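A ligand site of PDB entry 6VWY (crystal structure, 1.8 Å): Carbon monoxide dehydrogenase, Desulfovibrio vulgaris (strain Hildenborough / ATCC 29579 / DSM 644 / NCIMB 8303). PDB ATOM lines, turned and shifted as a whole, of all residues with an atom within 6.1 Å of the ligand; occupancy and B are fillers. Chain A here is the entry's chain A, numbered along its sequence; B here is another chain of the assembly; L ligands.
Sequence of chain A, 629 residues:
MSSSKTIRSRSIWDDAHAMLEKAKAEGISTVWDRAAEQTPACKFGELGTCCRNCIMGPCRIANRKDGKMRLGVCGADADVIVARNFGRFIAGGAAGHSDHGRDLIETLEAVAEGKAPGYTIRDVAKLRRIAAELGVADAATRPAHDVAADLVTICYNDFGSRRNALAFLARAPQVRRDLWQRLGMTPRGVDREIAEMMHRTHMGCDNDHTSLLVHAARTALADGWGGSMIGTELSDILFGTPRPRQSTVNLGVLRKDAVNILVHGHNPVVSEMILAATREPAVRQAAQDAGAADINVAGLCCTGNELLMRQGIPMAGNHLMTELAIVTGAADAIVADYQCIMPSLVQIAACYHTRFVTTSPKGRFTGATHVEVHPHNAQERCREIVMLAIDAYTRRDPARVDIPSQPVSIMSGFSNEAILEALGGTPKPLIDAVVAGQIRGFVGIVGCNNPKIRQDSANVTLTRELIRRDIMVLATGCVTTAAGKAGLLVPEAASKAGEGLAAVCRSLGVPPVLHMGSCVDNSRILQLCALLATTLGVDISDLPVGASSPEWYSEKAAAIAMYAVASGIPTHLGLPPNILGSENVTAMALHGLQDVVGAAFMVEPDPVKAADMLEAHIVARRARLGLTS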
ATOM      1  N   HIS A  97     -12.500  11.814 -14.094  1.00  0.00           N
ATOM      2  CA  HIS A  97     -11.381  11.971 -13.169  1.00  0.00           C
ATOM      3  C   HIS A  97     -10.038  11.946 -13.881  1.00  0.00           C
ATOM      4  O   HIS A  97      -9.115  12.676 -13.502  1.00  0.00           O
ATOM      5  CB  HIS A  97     -11.435  10.889 -12.098  1.00  0.00           C
ATOM      6  CG  HIS A  97     -12.607  11.004 -11.186  1.00  0.00           C
ATOM      7  ND1 HIS A  97     -13.366   9.917 -10.802  1.00  0.00           N
ATOM      8  CD2 HIS A  97     -13.165  12.088 -10.582  1.00  0.00           C
ATOM      9  CE1 HIS A  97     -14.332  10.318  -9.996  1.00  0.00           C
ATOM     10  NE2 HIS A  97     -14.230  11.633  -9.846  1.00  0.00           N
ATOM     11  N   GLY A 265     -17.573  23.339 -10.306  1.00  0.00           N
ATOM     12  CA  GLY A 265     -16.811  22.372 -11.074  1.00  0.00           C
ATOM     13  C   GLY A 265     -15.859  21.590 -10.180  1.00  0.00           C
ATOM     14  O   GLY A 265     -16.189  21.263  -9.044  1.00  0.00           O
ATOM     15  N   HIS A 266     -14.663  21.311 -10.715  1.00  0.00           N
ATOM     16  CA  HIS A 266     -13.735  20.374 -10.089  1.00  0.00           C
ATOM     17  C   HIS A 266     -12.288  20.841 -10.018  1.00  0.00           C
ATOM     18  O   HIS A 266     -11.566  20.374  -9.124  1.00  0.00           O
ATOM     19  CB  HIS A 266     -13.786  19.015 -10.823  1.00  0.00           C
ATOM     20  CG  HIS A 266     -14.875  18.104 -10.346  1.00  0.00           C
ATOM     21  ND1 HIS A 266     -16.208  18.353 -10.598  1.00  0.00           N
ATOM     22  CD2 HIS A 266     -14.837  16.982  -9.595  1.00  0.00           C
ATOM     23  CE1 HIS A 266     -16.946  17.407 -10.030  1.00  0.00           C
ATOM     24  NE2 HIS A 266     -16.141  16.558  -9.421  1.00  0.00           N
ATOM     25  N   CYS A 301     -19.748  22.320  -5.039  1.00  0.00           N
ATOM     26  CA  CYS A 301     -19.316  20.975  -5.415  1.00  0.00           C
ATOM     27  C   CYS A 301     -17.816  20.789  -5.196  1.00  0.00           C
ATOM     28  O   CYS A 301     -17.280  21.272  -4.201  1.00  0.00           O
ATOM     29  CB  CYS A 301     -19.773  20.684  -6.840  1.00  0.00           C
ATOM     30  SG  CYS A 301     -21.611  20.633  -6.928  1.00  0.00           S
ATOM     31  N   CYS A 302     -17.133  20.090  -6.098  1.00  0.00           N
ATOM     32  CA  CYS A 302     -15.809  19.606  -5.743  1.00  0.00           C
ATOM     33  C   CYS A 302     -14.734  20.671  -5.821  1.00  0.00           C
ATOM     34  O   CYS A 302     -13.750  20.600  -5.075  1.00  0.00           O
ATOM     35  CB  CYS A 302     -15.455  18.401  -6.591  1.00  0.00           C
ATOM     36  SG  CYS A 302     -16.353  16.957  -5.999  1.00  0.00           S
ATOM     37  N   ASN A 318     -24.126  21.942  -2.234  1.00  0.00           N
ATOM     38  CA  ASN A 318     -23.812  20.766  -3.020  1.00  0.00           C
ATOM     39  C   ASN A 318     -24.696  20.734  -4.269  1.00  0.00           C
ATOM     40  O   ASN A 318     -25.378  21.702  -4.588  1.00  0.00           O
ATOM     41  CB  ASN A 318     -23.934  19.492  -2.158  1.00  0.00           C
ATOM     42  CG  ASN A 318     -25.249  19.401  -1.407  1.00  0.00           C
ATOM     43  OD1 ASN A 318     -26.151  20.205  -1.610  1.00  0.00           O
ATOM     44  ND2 ASN A 318     -25.370  18.385  -0.531  1.00  0.00           N
ATOM     45  N   HIS A 319     -24.652  19.601  -4.987  1.00  0.00           N
ATOM     46  CA  HIS A 319     -25.237  19.458  -6.324  1.00  0.00           C
ATOM     47  C   HIS A 319     -26.634  20.082  -6.455  1.00  0.00           C
ATOM     48  O   HIS A 319     -26.830  20.979  -7.284  1.00  0.00           O
ATOM     49  CB  HIS A 319     -25.251  17.959  -6.670  1.00  0.00           C
ATOM     50  CG  HIS A 319     -25.981  17.604  -7.930  1.00  0.00           C
ATOM     51  ND1 HIS A 319     -25.852  18.320  -9.094  1.00  0.00           N
ATOM     52  CD2 HIS A 319     -26.812  16.570  -8.204  1.00  0.00           C
ATOM     53  CE1 HIS A 319     -26.599  17.756 -10.038  1.00  0.00           C
ATOM     54  NE2 HIS A 319     -27.199  16.697  -9.515  1.00  0.00           N
ATOM     55  N   GLN A 339     -17.513  19.461 -15.225  1.00  0.00           N
ATOM     56  CA  GLN A 339     -18.137  18.294 -14.597  1.00  0.00           C
ATOM     57  C   GLN A 339     -19.191  18.660 -13.559  1.00  0.00           C
ATOM     58  O   GLN A 339     -18.933  19.482 -12.680  1.00  0.00           O
ATOM     59  CB  GLN A 339     -17.109  17.362 -13.947  1.00  0.00           C
ATOM     60  CG  GLN A 339     -16.093  16.752 -14.885  1.00  0.00           C
ATOM     61  CD  GLN A 339     -14.995  16.085 -14.081  1.00  0.00           C
ATOM     62  OE1 GLN A 339     -15.136  15.847 -12.881  1.00  0.00           O
ATOM     63  NE2 GLN A 339     -13.870  15.809 -14.735  1.00  0.00           N
ATOM     64  N   CYS A 340     -20.376  18.055 -13.668  1.00  0.00           N
ATOM     65  CA  CYS A 340     -21.516  18.241 -12.762  1.00  0.00           C
ATOM     66  C   CYS A 340     -22.084  19.650 -12.792  1.00  0.00           C
ATOM     67  O   CYS A 340     -22.895  20.002 -11.920  1.00  0.00           O
ATOM     68  CB  CYS A 340     -21.162  17.846 -11.319  1.00  0.00           C
ATOM     69  SG  CYS A 340     -20.549  16.166 -11.166  1.00  0.00           S
ATOM     70  N   VAL A 446     -19.785   9.069   0.373  1.00  0.00           N
ATOM     71  CA  VAL A 446     -19.280   9.800  -0.766  1.00  0.00           C
ATOM     72  C   VAL A 446     -20.447  10.062  -1.715  1.00  0.00           C
ATOM     73  O   VAL A 446     -21.555   9.591  -1.491  1.00  0.00           O
ATOM     74  CB  VAL A 446     -18.147   9.028  -1.468  1.00  0.00           C
ATOM     75  CG1 VAL A 446     -17.152   8.519  -0.427  1.00  0.00           C
ATOM     76  CG2 VAL A 446     -18.728   7.842  -2.215  1.00  0.00           C
ATOM     77  N   GLY A 447     -20.208  10.784  -2.771  1.00  0.00           N
ATOM     78  CA  GLY A 447     -21.303  10.849  -3.726  1.00  0.00           C
ATOM     79  C   GLY A 447     -22.269  12.007  -3.519  1.00  0.00           C
ATOM     80  O   GLY A 447     -22.103  12.896  -2.683  1.00  0.00           O
ATOM     81  N   CYS A 448     -23.339  11.963  -4.328  1.00  0.00           N
ATOM     82  CA  CYS A 448     -24.004  13.153  -4.827  1.00  0.00           C
ATOM     83  C   CYS A 448     -25.359  13.380  -4.156  1.00  0.00           C
ATOM     84  O   CYS A 448     -25.623  12.885  -3.044  1.00  0.00           O
ATOM     85  CB  CYS A 448     -24.171  13.000  -6.352  1.00  0.00           C
ATOM     86  SG  CYS A 448     -22.910  12.033  -7.234  1.00  0.00           S
ATOM     87  N   ASN A 449     -26.187  14.170  -4.819  1.00  0.00           N
ATOM     88  CA  ASN A 449     -27.621  14.262  -4.596  1.00  0.00           C
ATOM     89  C   ASN A 449     -28.273  13.700  -5.846  1.00  0.00           C
ATOM     90  O   ASN A 449     -27.630  13.627  -6.907  1.00  0.00           O
ATOM     91  CB  ASN A 449     -28.106  15.710  -4.421  1.00  0.00           C
ATOM     92  CG  ASN A 449     -27.614  16.377  -3.160  1.00  0.00           C
ATOM     93  OD1 ASN A 449     -27.292  17.562  -3.176  1.00  0.00           O
ATOM     94  ND2 ASN A 449     -27.604  15.635  -2.048  1.00  0.00           N
ATOM     95  N   THR A 476     -16.802  12.871   1.742  1.00  0.00           N
ATOM     96  CA  THR A 476     -16.275  13.566   0.557  1.00  0.00           C
ATOM     97  C   THR A 476     -17.423  13.987  -0.347  1.00  0.00           C
ATOM     98  O   THR A 476     -18.576  13.573  -0.180  1.00  0.00           O
ATOM     99  CB  THR A 476     -15.302  12.706  -0.259  1.00  0.00           C
ATOM    100  OG1 THR A 476     -16.006  11.557  -0.764  1.00  0.00           O
ATOM    101  CG2 THR A 476     -14.102  12.277   0.580  1.00  0.00           C
ATOM    102  N   GLY A 477     -17.094  14.820  -1.331  1.00  0.00           N
ATOM    103  CA  GLY A 477     -18.054  15.215  -2.346  1.00  0.00           C
ATOM    104  C   GLY A 477     -19.229  15.973  -1.763  1.00  0.00           C
ATOM    105  O   GLY A 477     -19.099  16.756  -0.815  1.00  0.00           O
ATOM    106  N   CYS A 478     -20.397  15.732  -2.328  1.00  0.00           N
ATOM    107  CA  CYS A 478     -21.566  16.488  -1.888  1.00  0.00           C
ATOM    108  C   CYS A 478     -22.149  15.968  -0.565  1.00  0.00           C
ATOM    109  O   CYS A 478     -23.093  16.576  -0.053  1.00  0.00           O
ATOM    110  CB  CYS A 478     -22.579  16.496  -3.031  1.00  0.00           C
ATOM    111  SG  CYS A 478     -21.959  17.500  -4.435  1.00  0.00           S
ATOM    112  N   VAL A 479     -21.582  14.908   0.010  1.00  0.00           N
ATOM    113  CA  VAL A 479     -21.908  14.515   1.380  1.00  0.00           C
ATOM    114  C   VAL A 479     -21.335  15.503   2.384  1.00  0.00           C
ATOM    115  O   VAL A 479     -21.893  15.709   3.470  1.00  0.00           O
ATOM    116  CB  VAL A 479     -21.410  13.082   1.655  1.00  0.00           C
ATOM    117  CG1 VAL A 479     -21.686  12.656   3.121  1.00  0.00           C
ATOM    118  CG2 VAL A 479     -22.081  12.124   0.701  1.00  0.00           C
ATOM    119  N   SER A 518     -12.702  16.362  -1.977  1.00  0.00           N
ATOM    120  CA  SER A 518     -13.555  16.260  -3.159  1.00  0.00           C
ATOM    121  C   SER A 518     -13.688  14.799  -3.607  1.00  0.00           C
ATOM    122  O   SER A 518     -13.199  13.867  -2.978  1.00  0.00           O
ATOM    123  CB  SER A 518     -12.948  17.084  -4.282  1.00  0.00           C
ATOM    124  OG  SER A 518     -11.701  16.492  -4.623  1.00  0.00           O
ATOM    125  N   CYS A 519     -14.352  14.614  -4.747  1.00  0.00           N
ATOM    126  CA  CYS A 519     -14.533  13.273  -5.299  1.00  0.00           C
ATOM    127  C   CYS A 519     -13.202  12.649  -5.710  1.00  0.00           C
ATOM    128  O   CYS A 519     -13.025  11.437  -5.559  1.00  0.00           O
ATOM    129  CB  CYS A 519     -15.485  13.328  -6.488  1.00  0.00           C
ATOM    130  SG  CYS A 519     -17.143  13.592  -5.953  1.00  0.00           S
ATOM    131  N   TYR A 553     -25.709  10.108  -8.491  1.00  0.00           N
ATOM    132  CA  TYR A 553     -26.293  10.294  -9.818  1.00  0.00           C
ATOM    133  C   TYR A 553     -25.291  10.101 -10.961  1.00  0.00           C
ATOM    134  O   TYR A 553     -25.676   9.634 -12.037  1.00  0.00           O
ATOM    135  CB  TYR A 553     -26.953  11.709  -9.932  1.00  0.00           C
ATOM    136  CG  TYR A 553     -26.034  12.705 -10.558  1.00  0.00           C
ATOM    137  CD1 TYR A 553     -25.962  12.810 -11.942  1.00  0.00           C
ATOM    138  CD2 TYR A 553     -25.170  13.494  -9.785  1.00  0.00           C
ATOM    139  CE1 TYR A 553     -25.071  13.659 -12.550  1.00  0.00           C
ATOM    140  CE2 TYR A 553     -24.267  14.364 -10.398  1.00  0.00           C
ATOM    141  CZ  TYR A 553     -24.228  14.421 -11.786  1.00  0.00           C
ATOM    142  OH  TYR A 553     -23.344  15.227 -12.444  1.00  0.00           O
ATOM    143  N   SER A 554     -24.006  10.401 -10.777  1.00  0.00           N
ATOM    144  CA  SER A 554     -23.081  10.589 -11.880  1.00  0.00           C
ATOM    145  C   SER A 554     -22.372   9.293 -12.268  1.00  0.00           C
ATOM    146  O   SER A 554     -22.252   8.362 -11.466  1.00  0.00           O
ATOM    147  CB  SER A 554     -22.030  11.649 -11.533  1.00  0.00           C
ATOM    148  OG  SER A 554     -21.233  11.191 -10.450  1.00  0.00           O
ATOM    149  N   LYS A 556     -19.212   9.416 -12.592  1.00  0.00           N
ATOM    150  CA  LYS A 556     -18.037   9.490 -11.721  1.00  0.00           C
ATOM    151  C   LYS A 556     -18.287   8.759 -10.413  1.00  0.00           C
ATOM    152  O   LYS A 556     -17.431   8.005  -9.929  1.00  0.00           O
ATOM    153  CB  LYS A 556     -17.659  10.947 -11.483  1.00  0.00           C
ATOM    154  CG  LYS A 556     -16.957  11.600 -12.682  1.00  0.00           C
ATOM    155  CD  LYS A 556     -16.630  13.051 -12.427  1.00  0.00           C
ATOM    156  CE  LYS A 556     -17.889  13.853 -12.185  1.00  0.00           C
ATOM    157  NZ  LYS A 556     -17.855  14.577 -10.879  1.00  0.00           N
ATOM    158  N   ALA A 557     -19.470   8.959  -9.809  1.00  0.00           N
ATOM    159  CA  ALA A 557     -19.799   8.258  -8.574  1.00  0.00           C
ATOM    160  C   ALA A 557     -19.846   6.748  -8.774  1.00  0.00           C
ATOM    161  O   ALA A 557     -19.470   5.983  -7.873  1.00  0.00           O
ATOM    162  CB  ALA A 557     -21.129   8.774  -8.030  1.00  0.00           C
ATOM    163  N   ILE A 560     -16.273   5.524  -8.820  1.00  0.00           N
ATOM    164  CA  ILE A 560     -15.749   5.474  -7.456  1.00  0.00           C
ATOM    165  C   ILE A 560     -16.236   4.229  -6.734  1.00  0.00           C
ATOM    166  O   ILE A 560     -15.456   3.505  -6.109  1.00  0.00           O
ATOM    167  CB  ILE A 560     -16.152   6.761  -6.698  1.00  0.00           C
ATOM    168  CG1 ILE A 560     -15.381   7.962  -7.267  1.00  0.00           C
ATOM    169  CG2 ILE A 560     -15.931   6.565  -5.183  1.00  0.00           C
ATOM    170  CD1 ILE A 560     -16.023   9.340  -6.930  1.00  0.00           C
ATOM    171  N   HIS B 202     -19.658  13.455 -20.166  1.00  0.00           N
ATOM    172  CA  HIS B 202     -20.211  13.344 -18.819  1.00  0.00           C
ATOM    173  C   HIS B 202     -21.169  14.499 -18.554  1.00  0.00           C
ATOM    174  O   HIS B 202     -21.021  15.581 -19.120  1.00  0.00           O
ATOM    175  CB  HIS B 202     -19.065  13.355 -17.785  1.00  0.00           C
ATOM    176  CG  HIS B 202     -19.475  12.979 -16.393  1.00  0.00           C
ATOM    177  ND1 HIS B 202     -20.105  13.857 -15.537  1.00  0.00           N
ATOM    178  CD2 HIS B 202     -19.318  11.828 -15.699  1.00  0.00           C
ATOM    179  CE1 HIS B 202     -20.317  13.266 -14.383  1.00  0.00           C
ATOM    180  NE2 HIS B 202     -19.854  12.029 -14.448  1.00  0.00           N
HETATM  181 FE1  LIG L   1     -20.578  15.620  -8.959  1.00  0.00          FE
HETATM  182 FE2  LIG L   1     -17.620  16.264  -7.689  1.00  0.00          FE
HETATM  183 FE3  LIG L   1     -21.382  13.741  -7.294  1.00  0.00          FE
HETATM  184 FE4  LIG L   1     -21.205  16.082  -6.039  1.00  0.00          FE
HETATM  185  S1  LIG L   1     -20.326  14.068  -5.204  1.00  0.00           S
HETATM  186  S2  LIG L   1     -22.537  15.702  -7.765  1.00  0.00           S
HETATM  187  S3  LIG L   1     -19.903  13.422  -8.967  1.00  0.00           S
HETATM  188  S4  LIG L   1     -19.676  17.289  -7.515  1.00  0.00           S
HETATM  189 NI1  LIG L   1     -18.948  14.378  -6.970  1.00  0.00          NI
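S1 of the ligand sits close to O of Gly 447.
Merely in contact with the ligand: Cys 301 (3.5 Å), His 319 (3.7 Å), Gly 477 (3.8 Å) and Tyr 553 (3.4 Å).
Hydrophobic or aromatic side chains that line the ligand: His 266, His 319 and Tyr 553.
Within 4 Å of the ligand: His 266, Cys 301, Cys 302, His 319, Cys 340, Gly 447, Cys 448, Gly 477, Cys 478, Cys 519, Tyr 553, Ser 554 and Lys 556.
The nearest printed residue that does not touch the ligand is Ala 557 (4.6 Å).
NE2 of His 266 binds FE2 of the ligand, at 2.3 Å.
SG of Cys 340 is bound to FE1 of the ligand (2.3 Å).
A nickel atom (NI1) of the ligand is bound by the side-chain sulfur of Cys 519 (2.2 Å).
The backbone NH (N) of Cys 448 lies close to a sulfur (S1) of the ligand (3.8 Å).
A sulfur (S3) of the ligand sits close to the side-chain amino group of Lys 556 (3.0 Å).
A sulfur (S1) of the ligand lies close to the backbone NH (N) of Cys 478.
SG of Cys 302 binds FE2 of the ligand (2.2 Å).
The side-chain hydroxyl (OG) of Ser 554 lies close to a sulfur (S3) of the ligand (3.0 Å).
FE4 of the ligand is bound by SG of Cys 478, at 2.3 Å.
The side-chain sulfur (SG) of Cys 448 is bound to an iron atom (FE3) of the ligand (2.3 Å).
OH of Tyr 553 lies close to SG of Cys 340 (3.2 Å).
N of His 319 sits close to SG of Cys 478 (3.5 Å).
The side-chain sulfur (SG) of Cys 301 sits at hydrogen-bond distance from the backbone NH (N) of His 319 (3.8 Å).
The side-chain sulfur (SG) of Cys 302 sits close to the backbone NH (N) of Cys 519 (3.3 Å).
The backbone NH (N) of Cys 302 sits at hydrogen-bond distance from the backbone carbonyl oxygen (O) of Gly 265, 3.3 Å away.
The backbone NH (N) of Cys 478 lies within hydrogen-bond range of the backbone carbonyl oxygen (O) of Gly 447 (3.3 Å).
SG of Cys 340 sits close to NZ of Lys 556 (3.1 Å).
The backbone NH of Lys 556 lies within hydrogen-bond range of a ring nitrogen (NE2) of His 202 of chain B, at 3.3 Å.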
